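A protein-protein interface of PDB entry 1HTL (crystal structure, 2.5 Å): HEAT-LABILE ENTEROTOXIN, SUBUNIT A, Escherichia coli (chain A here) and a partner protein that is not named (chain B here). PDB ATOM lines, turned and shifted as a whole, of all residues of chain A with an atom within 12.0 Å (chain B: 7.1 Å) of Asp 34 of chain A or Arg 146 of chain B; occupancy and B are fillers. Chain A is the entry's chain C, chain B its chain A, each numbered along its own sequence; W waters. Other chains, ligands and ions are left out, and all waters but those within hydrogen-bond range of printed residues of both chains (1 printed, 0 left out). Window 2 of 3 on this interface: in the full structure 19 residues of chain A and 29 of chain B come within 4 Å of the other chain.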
ATOM      1  N   TYR A  23     -36.719   9.883  21.078  1.00  0.00           N
ATOM      2  CA  TYR A  23     -35.578  10.793  21.021  1.00  0.00           C
ATOM      3  C   TYR A  23     -35.672  11.814  22.173  1.00  0.00           C
ATOM      4  O   TYR A  23     -34.660  12.139  22.792  1.00  0.00           O
ATOM      5  CB  TYR A  23     -35.482  11.479  19.660  1.00  0.00           C
ATOM      6  CG  TYR A  23     -34.263  12.335  19.537  1.00  0.00           C
ATOM      7  CD1 TYR A  23     -33.019  11.774  19.287  1.00  0.00           C
ATOM      8  CD2 TYR A  23     -34.347  13.718  19.688  1.00  0.00           C
ATOM      9  CE1 TYR A  23     -31.892  12.566  19.192  1.00  0.00           C
ATOM     10  CE2 TYR A  23     -33.232  14.510  19.593  1.00  0.00           C
ATOM     11  CZ  TYR A  23     -32.008  13.939  19.346  1.00  0.00           C
ATOM     12  OH  TYR A  23     -30.903  14.756  19.223  1.00  0.00           O
ATOM     13  N   GLN A  24     -36.896  12.224  22.512  1.00  0.00           N
ATOM     14  CA  GLN A  24     -37.178  13.160  23.612  1.00  0.00           C
ATOM     15  C   GLN A  24     -36.822  12.563  24.966  1.00  0.00           C
ATOM     16  O   GLN A  24     -36.707  13.287  25.963  1.00  0.00           O
ATOM     17  CB  GLN A  24     -38.644  13.573  23.635  1.00  0.00           C
ATOM     18  CG  GLN A  24     -39.016  14.570  22.569  1.00  0.00           C
ATOM     19  CD  GLN A  24     -40.412  15.117  22.749  1.00  0.00           C
ATOM     20  OE1 GLN A  24     -41.238  14.496  23.405  1.00  0.00           O
ATOM     21  NE2 GLN A  24     -40.695  16.258  22.142  1.00  0.00           N
ATOM     22  N   SER A  25     -36.668  11.239  24.992  1.00  0.00           N
ATOM     23  CA  SER A  25     -36.264  10.504  26.195  1.00  0.00           C
ATOM     24  C   SER A  25     -34.711  10.431  26.268  1.00  0.00           C
ATOM     25  O   SER A  25     -34.135  10.474  27.357  1.00  0.00           O
ATOM     26  CB  SER A  25     -36.880   9.108  26.203  1.00  0.00           C
ATOM     27  OG  SER A  25     -36.885   8.604  27.513  1.00  0.00           O
ATOM     28  N   LYS A  26     -34.038  10.345  25.114  1.00  0.00           N
ATOM     29  CA  LYS A  26     -32.569  10.341  25.095  1.00  0.00           C
ATOM     30  C   LYS A  26     -32.199  11.688  25.698  1.00  0.00           C
ATOM     31  O   LYS A  26     -31.486  11.773  26.696  1.00  0.00           O
ATOM     32  CB  LYS A  26     -32.002  10.310  23.667  1.00  0.00           C
ATOM     33  CG  LYS A  26     -32.146   9.017  22.898  1.00  0.00           C
ATOM     34  CD  LYS A  26     -31.797   7.804  23.725  1.00  0.00           C
ATOM     35  CE  LYS A  26     -31.486   6.626  22.827  1.00  0.00           C
ATOM     36  NZ  LYS A  26     -31.450   5.345  23.598  1.00  0.00           N
ATOM     37  N   VAL A  27     -32.733  12.749  25.106  1.00  0.00           N
ATOM     38  CA  VAL A  27     -32.471  14.100  25.584  1.00  0.00           C
ATOM     39  C   VAL A  27     -32.784  14.226  27.088  1.00  0.00           C
ATOM     40  O   VAL A  27     -31.942  14.685  27.849  1.00  0.00           O
ATOM     41  CB  VAL A  27     -33.245  15.136  24.736  1.00  0.00           C
ATOM     42  CG1 VAL A  27     -33.220  16.492  25.397  1.00  0.00           C
ATOM     43  CG2 VAL A  27     -32.628  15.225  23.352  1.00  0.00           C
ATOM     44  N   LYS A  28     -33.951  13.775  27.541  1.00  0.00           N
ATOM     45  CA  LYS A  28     -34.248  13.857  28.971  1.00  0.00           C
ATOM     46  C   LYS A  28     -33.225  13.090  29.817  1.00  0.00           C
ATOM     47  O   LYS A  28     -32.950  13.468  30.960  1.00  0.00           O
ATOM     48  CB  LYS A  28     -35.639  13.319  29.287  1.00  0.00           C
ATOM     49  CG  LYS A  28     -36.794  14.277  28.987  1.00  0.00           C
ATOM     50  CD  LYS A  28     -37.955  13.966  29.917  1.00  0.00           C
ATOM     51  CE  LYS A  28     -39.119  14.887  29.764  1.00  0.00           C
ATOM     52  NZ  LYS A  28     -40.193  14.407  30.732  1.00  0.00           N
ATOM     53  N   ARG A  29     -32.690  11.991  29.282  1.00  0.00           N
ATOM     54  CA  ARG A  29     -31.715  11.177  30.014  1.00  0.00           C
ATOM     55  C   ARG A  29     -30.421  11.919  30.173  1.00  0.00           C
ATOM     56  O   ARG A  29     -29.659  11.658  31.084  1.00  0.00           O
ATOM     57  CB  ARG A  29     -31.480   9.823  29.326  1.00  0.00           C
ATOM     58  CG  ARG A  29     -32.541   8.776  29.693  1.00  0.00           C
ATOM     59  CD  ARG A  29     -32.591   7.573  28.760  1.00  0.00           C
ATOM     60  NE  ARG A  29     -31.350   6.808  28.738  1.00  0.00           N
ATOM     61  CZ  ARG A  29     -31.222   5.593  28.217  1.00  0.00           C
ATOM     62  NH1 ARG A  29     -32.263   4.984  27.670  1.00  0.00           N
ATOM     63  NH2 ARG A  29     -30.057   4.980  28.254  1.00  0.00           N
ATOM     64  N   GLN A  30     -30.169  12.847  29.266  1.00  0.00           N
ATOM     65  CA  GLN A  30     -28.974  13.661  29.316  1.00  0.00           C
ATOM     66  C   GLN A  30     -29.142  14.724  30.395  1.00  0.00           C
ATOM     67  O   GLN A  30     -28.509  14.652  31.457  1.00  0.00           O
ATOM     68  CB  GLN A  30     -28.754  14.372  27.969  1.00  0.00           C
ATOM     69  CG  GLN A  30     -28.112  13.527  26.893  1.00  0.00           C
ATOM     70  CD  GLN A  30     -26.921  12.772  27.414  1.00  0.00           C
ATOM     71  OE1 GLN A  30     -25.952  13.372  27.885  1.00  0.00           O
ATOM     72  NE2 GLN A  30     -26.991  11.457  27.368  1.00  0.00           N
ATOM     73  N   ILE A  31     -30.067  15.657  30.134  1.00  0.00           N
ATOM     74  CA  ILE A  31     -30.344  16.819  30.983  1.00  0.00           C
ATOM     75  C   ILE A  31     -30.958  16.674  32.390  1.00  0.00           C
ATOM     76  O   ILE A  31     -30.580  17.402  33.296  1.00  0.00           O
ATOM     77  CB  ILE A  31     -31.112  17.914  30.171  1.00  0.00           C
ATOM     78  CG1 ILE A  31     -32.533  17.462  29.852  1.00  0.00           C
ATOM     79  CG2 ILE A  31     -30.393  18.200  28.846  1.00  0.00           C
ATOM     80  CD1 ILE A  31     -33.334  18.469  29.064  1.00  0.00           C
ATOM     81  N   PHE A  32     -31.874  15.739  32.593  1.00  0.00           N
ATOM     82  CA  PHE A  32     -32.486  15.566  33.904  1.00  0.00           C
ATOM     83  C   PHE A  32     -31.549  14.812  34.845  1.00  0.00           C
ATOM     84  O   PHE A  32     -31.715  14.855  36.055  1.00  0.00           O
ATOM     85  CB  PHE A  32     -33.838  14.824  33.790  1.00  0.00           C
ATOM     86  CG  PHE A  32     -34.965  15.656  33.187  1.00  0.00           C
ATOM     87  CD1 PHE A  32     -34.738  16.943  32.696  1.00  0.00           C
ATOM     88  CD2 PHE A  32     -36.267  15.152  33.139  1.00  0.00           C
ATOM     89  CE1 PHE A  32     -35.777  17.705  32.175  1.00  0.00           C
ATOM     90  CE2 PHE A  32     -37.319  15.910  32.622  1.00  0.00           C
ATOM     91  CZ  PHE A  32     -37.075  17.186  32.141  1.00  0.00           C
ATOM     92  N   SER A  33     -30.580  14.100  34.288  1.00  0.00           N
ATOM     93  CA  SER A  33     -29.619  13.350  35.101  1.00  0.00           C
ATOM     94  C   SER A  33     -28.651  14.262  35.841  1.00  0.00           C
ATOM     95  O   SER A  33     -28.053  13.851  36.826  1.00  0.00           O
ATOM     96  CB  SER A  33     -28.861  12.326  34.255  1.00  0.00           C
ATOM     97  OG  SER A  33     -29.765  11.324  33.794  1.00  0.00           O
ATOM     98  N   ASP A  34     -28.501  15.505  35.385  1.00  0.00           N
ATOM     99  CA  ASP A  34     -27.616  16.455  36.069  1.00  0.00           C
ATOM    100  C   ASP A  34     -28.125  16.676  37.487  1.00  0.00           C
ATOM    101  O   ASP A  34     -27.352  16.904  38.425  1.00  0.00           O
ATOM    102  CB  ASP A  34     -27.612  17.804  35.352  1.00  0.00           C
ATOM    103  CG  ASP A  34     -26.953  17.738  34.000  1.00  0.00           C
ATOM    104  OD1 ASP A  34     -26.135  16.826  33.770  1.00  0.00           O
ATOM    105  OD2 ASP A  34     -27.261  18.596  33.153  1.00  0.00           O
ATOM    106  N   TYR A  35     -29.444  16.591  37.622  1.00  0.00           N
ATOM    107  CA  TYR A  35     -30.104  16.805  38.889  1.00  0.00           C
ATOM    108  C   TYR A  35     -30.167  15.601  39.820  1.00  0.00           C
ATOM    109  O   TYR A  35     -30.590  15.728  40.951  1.00  0.00           O
ATOM    110  CB  TYR A  35     -31.495  17.385  38.638  1.00  0.00           C
ATOM    111  CG  TYR A  35     -31.513  18.581  37.685  1.00  0.00           C
ATOM    112  CD1 TYR A  35     -31.153  19.853  38.117  1.00  0.00           C
ATOM    113  CD2 TYR A  35     -31.900  18.441  36.364  1.00  0.00           C
ATOM    114  CE1 TYR A  35     -31.182  20.966  37.236  1.00  0.00           C
ATOM    115  CE2 TYR A  35     -31.934  19.527  35.486  1.00  0.00           C
ATOM    116  CZ  TYR A  35     -31.575  20.787  35.925  1.00  0.00           C
ATOM    117  OH  TYR A  35     -31.594  21.864  35.056  1.00  0.00           O
ATOM    118  N   GLN A  36     -29.671  14.449  39.389  1.00  0.00           N
ATOM    119  CA  GLN A  36     -29.724  13.250  40.231  1.00  0.00           C
ATOM    120  C   GLN A  36     -28.692  13.244  41.352  1.00  0.00           C
ATOM    121  O   GLN A  36     -27.520  13.057  41.105  1.00  0.00           O
ATOM    122  CB  GLN A  36     -29.588  11.971  39.357  1.00  0.00           C
ATOM    123  CG  GLN A  36     -29.396  10.608  40.105  1.00  0.00           C
ATOM    124  CD  GLN A  36     -30.573  10.222  41.016  1.00  0.00           C
ATOM    125  OE1 GLN A  36     -30.377   9.680  42.107  1.00  0.00           O
ATOM    126  NE2 GLN A  36     -31.787  10.479  40.560  1.00  0.00           N
ATOM    127  N   SER A  37     -29.149  13.396  42.583  1.00  0.00           N
ATOM    128  CA  SER A  37     -28.273  13.411  43.749  1.00  0.00           C
ATOM    129  C   SER A  37     -28.263  12.030  44.377  1.00  0.00           C
ATOM    130  O   SER A  37     -29.278  11.586  44.886  1.00  0.00           O
ATOM    131  CB  SER A  37     -28.793  14.431  44.779  1.00  0.00           C
ATOM    132  OG  SER A  37     -28.083  14.379  46.012  1.00  0.00           O
ATOM    133  N   GLU A  38     -27.107  11.375  44.412  1.00  0.00           N
ATOM    134  CA  GLU A  38     -27.045  10.050  45.016  1.00  0.00           C
ATOM    135  C   GLU A  38     -27.244  10.108  46.522  1.00  0.00           C
ATOM    136  O   GLU A  38     -27.136  11.167  47.144  1.00  0.00           O
ATOM    137  CB  GLU A  38     -25.760   9.294  44.657  1.00  0.00           C
ATOM    138  CG  GLU A  38     -25.523   9.075  43.143  1.00  0.00           C
ATOM    139  CD  GLU A  38     -26.775   8.736  42.296  1.00  0.00           C
ATOM    140  OE1 GLU A  38     -27.783   8.184  42.803  1.00  0.00           O
ATOM    141  OE2 GLU A  38     -26.734   9.034  41.086  1.00  0.00           O
ATOM    142  N   VAL A  39     -27.537   8.955  47.105  1.00  0.00           N
ATOM    143  CA  VAL A  39     -27.813   8.866  48.523  1.00  0.00           C
ATOM    144  C   VAL A  39     -26.893   7.874  49.192  1.00  0.00           C
ATOM    145  O   VAL A  39     -26.389   6.954  48.553  1.00  0.00           O
ATOM    146  CB  VAL A  39     -29.278   8.386  48.718  1.00  0.00           C
ATOM    147  CG1 VAL A  39     -29.589   8.135  50.182  1.00  0.00           C
ATOM    148  CG2 VAL A  39     -30.254   9.388  48.102  1.00  0.00           C
ATOM    149  N   ALA B  89     -25.459  20.548  16.059  1.00  0.00           N
ATOM    150  CA  ALA B  89     -24.695  19.342  15.867  1.00  0.00           C
ATOM    151  C   ALA B  89     -25.578  18.283  15.200  1.00  0.00           C
ATOM    152  O   ALA B  89     -26.809  18.405  15.201  1.00  0.00           O
ATOM    153  CB  ALA B  89     -24.172  18.863  17.196  1.00  0.00           C
ATOM    154  N   TYR B 121     -32.431  22.455  22.844  1.00  0.00           N
ATOM    155  CA  TYR B 121     -31.450  23.495  23.159  1.00  0.00           C
ATOM    156  C   TYR B 121     -30.063  22.912  23.444  1.00  0.00           C
ATOM    157  O   TYR B 121     -29.056  23.496  23.082  1.00  0.00           O
ATOM    158  CB  TYR B 121     -31.922  24.296  24.361  1.00  0.00           C
ATOM    159  CG  TYR B 121     -31.244  25.627  24.487  1.00  0.00           C
ATOM    160  CD1 TYR B 121     -31.409  26.602  23.511  1.00  0.00           C
ATOM    161  CD2 TYR B 121     -30.486  25.944  25.609  1.00  0.00           C
ATOM    162  CE1 TYR B 121     -30.848  27.869  23.651  1.00  0.00           C
ATOM    163  CE2 TYR B 121     -29.917  27.215  25.760  1.00  0.00           C
ATOM    164  CZ  TYR B 121     -30.114  28.177  24.776  1.00  0.00           C
ATOM    165  OH  TYR B 121     -29.657  29.470  24.954  1.00  0.00           O
ATOM    166  N   SER B 122     -30.018  21.741  24.066  1.00  0.00           N
ATOM    167  CA  SER B 122     -28.756  21.088  24.371  1.00  0.00           C
ATOM    168  C   SER B 122     -27.999  20.610  23.124  1.00  0.00           C
ATOM    169  O   SER B 122     -26.807  20.272  23.196  1.00  0.00           O
ATOM    170  CB  SER B 122     -28.989  19.925  25.333  1.00  0.00           C
ATOM    171  OG  SER B 122     -30.076  19.113  24.927  1.00  0.00           O
ATOM    172  N   GLN B 123     -28.682  20.608  21.983  1.00  0.00           N
ATOM    173  CA  GLN B 123     -28.084  20.170  20.723  1.00  0.00           C
ATOM    174  C   GLN B 123     -27.536  21.342  19.919  1.00  0.00           C
ATOM    175  O   GLN B 123     -26.934  21.167  18.861  1.00  0.00           O
ATOM    176  CB  GLN B 123     -29.134  19.433  19.885  1.00  0.00           C
ATOM    177  CG  GLN B 123     -28.584  18.688  18.679  1.00  0.00           C
ATOM    178  CD  GLN B 123     -29.645  17.900  17.944  1.00  0.00           C
ATOM    179  OE1 GLN B 123     -30.657  17.534  18.519  1.00  0.00           O
ATOM    180  NE2 GLN B 123     -29.411  17.626  16.665  1.00  0.00           N
ATOM    181  N   ILE B 124     -27.808  22.548  20.376  1.00  0.00           N
ATOM    182  CA  ILE B 124     -27.325  23.710  19.673  1.00  0.00           C
ATOM    183  C   ILE B 124     -25.903  24.088  20.119  1.00  0.00           C
ATOM    184  O   ILE B 124     -25.611  24.245  21.304  1.00  0.00           O
ATOM    185  CB  ILE B 124     -28.307  24.885  19.815  1.00  0.00           C
ATOM    186  CG1 ILE B 124     -29.616  24.541  19.094  1.00  0.00           C
ATOM    187  CG2 ILE B 124     -27.672  26.179  19.275  1.00  0.00           C
ATOM    188  CD1 ILE B 124     -30.598  25.645  19.102  1.00  0.00           C
ATOM    189  N   ASN B 142     -22.796  28.076  23.060  1.00  0.00           N
ATOM    190  CA  ASN B 142     -23.859  27.611  23.942  1.00  0.00           C
ATOM    191  C   ASN B 142     -23.268  26.706  25.037  1.00  0.00           C
ATOM    192  O   ASN B 142     -22.840  25.585  24.791  1.00  0.00           O
ATOM    193  CB  ASN B 142     -24.901  26.861  23.120  1.00  0.00           C
ATOM    194  CG  ASN B 142     -25.996  26.288  23.962  1.00  0.00           C
ATOM    195  OD1 ASN B 142     -26.055  26.536  25.161  1.00  0.00           O
ATOM    196  ND2 ASN B 142     -26.875  25.504  23.345  1.00  0.00           N
ATOM    197  N   ARG B 143     -23.294  27.203  26.263  1.00  0.00           N
ATOM    198  CA  ARG B 143     -22.747  26.499  27.416  1.00  0.00           C
ATOM    199  C   ARG B 143     -23.476  25.230  27.816  1.00  0.00           C
ATOM    200  O   ARG B 143     -22.956  24.437  28.598  1.00  0.00           O
ATOM    201  CB  ARG B 143     -22.658  27.441  28.627  1.00  0.00           C
ATOM    202  CG  ARG B 143     -23.954  28.167  29.006  1.00  0.00           C
ATOM    203  CD  ARG B 143     -24.218  29.400  28.133  1.00  0.00           C
ATOM    204  NE  ARG B 143     -25.482  29.295  27.402  1.00  0.00           N
ATOM    205  CZ  ARG B 143     -25.842  30.079  26.386  1.00  0.00           C
ATOM    206  NH1 ARG B 143     -25.041  31.049  25.949  1.00  0.00           N
ATOM    207  NH2 ARG B 143     -27.018  29.889  25.804  1.00  0.00           N
ATOM    208  N   GLU B 144     -24.695  25.063  27.314  1.00  0.00           N
ATOM    209  CA  GLU B 144     -25.498  23.886  27.620  1.00  0.00           C
ATOM    210  C   GLU B 144     -25.379  22.820  26.544  1.00  0.00           C
ATOM    211  O   GLU B 144     -26.045  21.786  26.600  1.00  0.00           O
ATOM    212  CB  GLU B 144     -26.956  24.279  27.846  1.00  0.00           C
ATOM    213  CG  GLU B 144     -27.210  24.784  29.262  1.00  0.00           C
ATOM    214  CD  GLU B 144     -28.510  25.541  29.409  1.00  0.00           C
ATOM    215  OE1 GLU B 144     -29.450  25.298  28.627  1.00  0.00           O
ATOM    216  OE2 GLU B 144     -28.588  26.394  30.314  1.00  0.00           O
ATOM    217  N   TYR B 145     -24.533  23.080  25.556  1.00  0.00           N
ATOM    218  CA  TYR B 145     -24.312  22.129  24.487  1.00  0.00           C
ATOM    219  C   TYR B 145     -23.651  20.907  25.119  1.00  0.00           C
ATOM    220  O   TYR B 145     -22.673  21.031  25.853  1.00  0.00           O
ATOM    221  CB  TYR B 145     -23.423  22.751  23.408  1.00  0.00           C
ATOM    222  CG  TYR B 145     -22.865  21.772  22.405  1.00  0.00           C
ATOM    223  CD1 TYR B 145     -23.656  21.265  21.369  1.00  0.00           C
ATOM    224  CD2 TYR B 145     -21.526  21.392  22.453  1.00  0.00           C
ATOM    225  CE1 TYR B 145     -23.110  20.397  20.390  1.00  0.00           C
ATOM    226  CE2 TYR B 145     -20.974  20.535  21.486  1.00  0.00           C
ATOM    227  CZ  TYR B 145     -21.760  20.042  20.457  1.00  0.00           C
ATOM    228  OH  TYR B 145     -21.188  19.211  19.502  1.00  0.00           O
ATOM    229  N   ARG B 146     -24.224  19.729  24.886  1.00  0.00           N
ATOM    230  CA  ARG B 146     -23.666  18.505  25.437  1.00  0.00           C
ATOM    231  C   ARG B 146     -22.697  17.953  24.413  1.00  0.00           C
ATOM    232  O   ARG B 146     -23.053  17.147  23.553  1.00  0.00           O
ATOM    233  CB  ARG B 146     -24.773  17.520  25.710  1.00  0.00           C
ATOM    234  CG  ARG B 146     -25.974  18.188  26.284  1.00  0.00           C
ATOM    235  CD  ARG B 146     -26.745  17.213  27.061  1.00  0.00           C
ATOM    236  NE  ARG B 146     -25.955  16.642  28.148  1.00  0.00           N
ATOM    237  CZ  ARG B 146     -25.964  17.117  29.392  1.00  0.00           C
ATOM    238  NH1 ARG B 146     -26.705  18.178  29.703  1.00  0.00           N
ATOM    239  NH2 ARG B 146     -25.302  16.481  30.347  1.00  0.00           N
ATOM    240  N   ASP B 147     -21.454  18.395  24.520  1.00  0.00           N
ATOM    241  CA  ASP B 147     -20.411  17.993  23.597  1.00  0.00           C
ATOM    242  C   ASP B 147     -20.137  16.503  23.565  1.00  0.00           C
ATOM    243  O   ASP B 147     -20.019  15.940  22.489  1.00  0.00           O
ATOM    244  CB  ASP B 147     -19.113  18.746  23.902  1.00  0.00           C
ATOM    245  CG  ASP B 147     -18.261  18.963  22.672  1.00  0.00           C
ATOM    246  OD1 ASP B 147     -17.781  17.991  22.054  1.00  0.00           O
ATOM    247  OD2 ASP B 147     -18.064  20.135  22.323  1.00  0.00           O
ATOM    248  N   ARG B 148     -20.017  15.856  24.719  1.00  0.00           N
ATOM    249  CA  ARG B 148     -19.714  14.435  24.691  1.00  0.00           C
ATOM    250  C   ARG B 148     -20.849  13.636  24.115  1.00  0.00           C
ATOM    251  O   ARG B 148     -20.610  12.618  23.487  1.00  0.00           O
ATOM    252  CB  ARG B 148     -19.381  13.864  26.057  1.00  0.00           C
ATOM    253  CG  ARG B 148     -19.072  12.349  25.979  1.00  0.00           C
ATOM    254  CD  ARG B 148     -19.130  11.624  27.326  1.00  0.00           C
ATOM    255  NE  ARG B 148     -18.083  12.089  28.222  1.00  0.00           N
ATOM    256  CZ  ARG B 148     -18.302  12.675  29.393  1.00  0.00           C
ATOM    257  NH1 ARG B 148     -19.544  12.865  29.834  1.00  0.00           N
ATOM    258  NH2 ARG B 148     -17.273  13.119  30.100  1.00  0.00           N
ATOM    259  N   TYR B 149     -22.085  14.083  24.323  1.00  0.00           N
ATOM    260  CA  TYR B 149     -23.204  13.330  23.806  1.00  0.00           C
ATOM    261  C   TYR B 149     -23.375  13.534  22.308  1.00  0.00           C
ATOM    262  O   TYR B 149     -23.513  12.554  21.581  1.00  0.00           O
ATOM    263  CB  TYR B 149     -24.476  13.668  24.566  1.00  0.00           C
ATOM    264  CG  TYR B 149     -25.689  12.886  24.133  1.00  0.00           C
ATOM    265  CD1 TYR B 149     -25.798  11.522  24.397  1.00  0.00           C
ATOM    266  CD2 TYR B 149     -26.724  13.508  23.426  1.00  0.00           C
ATOM    267  CE1 TYR B 149     -26.910  10.787  23.960  1.00  0.00           C
ATOM    268  CE2 TYR B 149     -27.838  12.790  22.985  1.00  0.00           C
ATOM    269  CZ  TYR B 149     -27.925  11.433  23.250  1.00  0.00           C
ATOM    270  OH  TYR B 149     -29.013  10.727  22.780  1.00  0.00           O
ATOM    271  N   TYR B 150     -23.289  14.775  21.829  1.00  0.00           N
ATOM    272  CA  TYR B 150     -23.464  15.032  20.401  1.00  0.00           C
ATOM    273  C   TYR B 150     -22.215  14.847  19.507  1.00  0.00           C
ATOM    274  O   TYR B 150     -22.311  14.841  18.264  1.00  0.00           O
ATOM    275  CB  TYR B 150     -24.116  16.394  20.194  1.00  0.00           C
ATOM    276  CG  TYR B 150     -25.513  16.491  20.800  1.00  0.00           C
ATOM    277  CD1 TYR B 150     -26.618  15.954  20.150  1.00  0.00           C
ATOM    278  CD2 TYR B 150     -25.714  17.076  22.041  1.00  0.00           C
ATOM    279  CE1 TYR B 150     -27.872  15.989  20.727  1.00  0.00           C
ATOM    280  CE2 TYR B 150     -26.955  17.119  22.621  1.00  0.00           C
ATOM    281  CZ  TYR B 150     -28.033  16.569  21.966  1.00  0.00           C
ATOM    282  OH  TYR B 150     -29.269  16.562  22.588  1.00  0.00           O
ATOM    283  N   ARG B 151     -21.067  14.617  20.146  1.00  0.00           N
ATOM    284  CA  ARG B 151     -19.783  14.417  19.469  1.00  0.00           C
ATOM    285  C   ARG B 151     -19.764  13.109  18.690  1.00  0.00           C
ATOM    286  O   ARG B 151     -19.205  13.035  17.597  1.00  0.00           O
ATOM    287  CB  ARG B 151     -18.634  14.396  20.493  1.00  0.00           C
ATOM    288  CG  ARG B 151     -17.210  14.227  19.900  1.00  0.00           C
ATOM    289  CD  ARG B 151     -16.090  14.253  20.970  1.00  0.00           C
ATOM    290  NE  ARG B 151     -16.244  15.353  21.932  1.00  0.00           N
ATOM    291  CZ  ARG B 151     -16.347  15.184  23.249  1.00  0.00           C
ATOM    292  NH1 ARG B 151     -16.293  13.959  23.763  1.00  0.00           N
ATOM    293  NH2 ARG B 151     -16.580  16.221  24.048  1.00  0.00           N
HETATM  294  O   HOH W   1     -22.909  12.772  28.909  1.00  0.00           O
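The side-chain carboxylate (OD2) of Asp 34 of chain A lies within salt-bridge range of the guanidinium group (NH1) of Arg 146 of chain B (3.5 Å).
OE1 of Gln 123 of chain B sits at hydrogen-bond distance from OH of Tyr 23 of chain A, at 2.9 Å.
The guanidinium group (NE) of Arg 146 of chain B lies within hydrogen-bond range of the side-chain amide oxygen (OE1) of Gln 30 of chain A, at 3.3 Å.
The side-chain amide nitrogen (NE2) of Gln 123 of chain B lies within hydrogen-bond range of the backbone carbonyl oxygen (O) of Ala 89 of chain B.
The backbone carbonyl oxygen (O) of Ser 122 of chain B lies within hydrogen-bond range of the backbone NH (N) of Arg 146 of chain B (3.1 Å).
Tyr 23 of chain A touches Tyr 150 of chain B (OH to CE1, 3.6 Å).
Tyr 149 of chain B touches Lys 26 of chain A.
Tyr 150 of chain B touches Val 27 of chain A (OH to CG2, 3.7 Å).
Gln 30 of chain A touches Tyr 149 of chain B (NE2 to CD1, 3.2 Å).
Ile 31 of chain A touches Arg 146 of chain B.
Asp 34 of chain A touches just one residue of chain B: Arg 146.
Printed residues of chain A within 4 Å of Arg 146 of chain B: Gln 30, Ile 31 and Asp 34.
No residue of chain A comes within 4 Å of Ser 122 of chain B.
No residue of chain A comes within 4 Å of Asp 147 of chain B.
Of chain A, only Tyr 23 (3.6 Å) and Val 27 (3.7 Å) come within 4 Å of Tyr 150 of chain B.
Of the printed residues of chain A, Tyr 149 of chain B touches Lys 26 (3.1 Å) and Gln 30 (3.2 Å).
Printed residues of chain B within 4 Å of Tyr 23 of chain A: Gln 123 (2.9 Å) and Tyr 150 (3.6 Å).
Of the printed residues of chain B, Ile 31 of chain A touches Arg 146.
Printed residues of chain B within 4 Å of Lys 26 of chain A: Tyr 149 (3.1 Å).
The nearest printed residue of chain B that does not touch Asp 34 of chain A is Glu 144 of chain B (7.3 Å).
Hydrophobic or aromatic side chains of chain A that line the printed part of chain B: Tyr 23, Val 27 and Ile 31.
Printed residues of chain B that touch a printed residue of chain A: Gln 123, Arg 146, Tyr 149 and Tyr 150.
Hydrophobic or aromatic side chains of chain B within 4 Å of the printed part of chain A: Tyr 149 and Tyr 150.
Among the printed residues, Asp or Glu carboxylates within 4 Å of a Lys or Arg side-chain nitrogen of the other chain: Asp 34 of chain A with Arg 146 of chain B.
Water W1 lies within hydrogen-bond range of the side-chain amide oxygen of Gln 30 of chain A (3.3 Å) and the guanidinium group of Arg 148 of chain B (3.5 Å).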
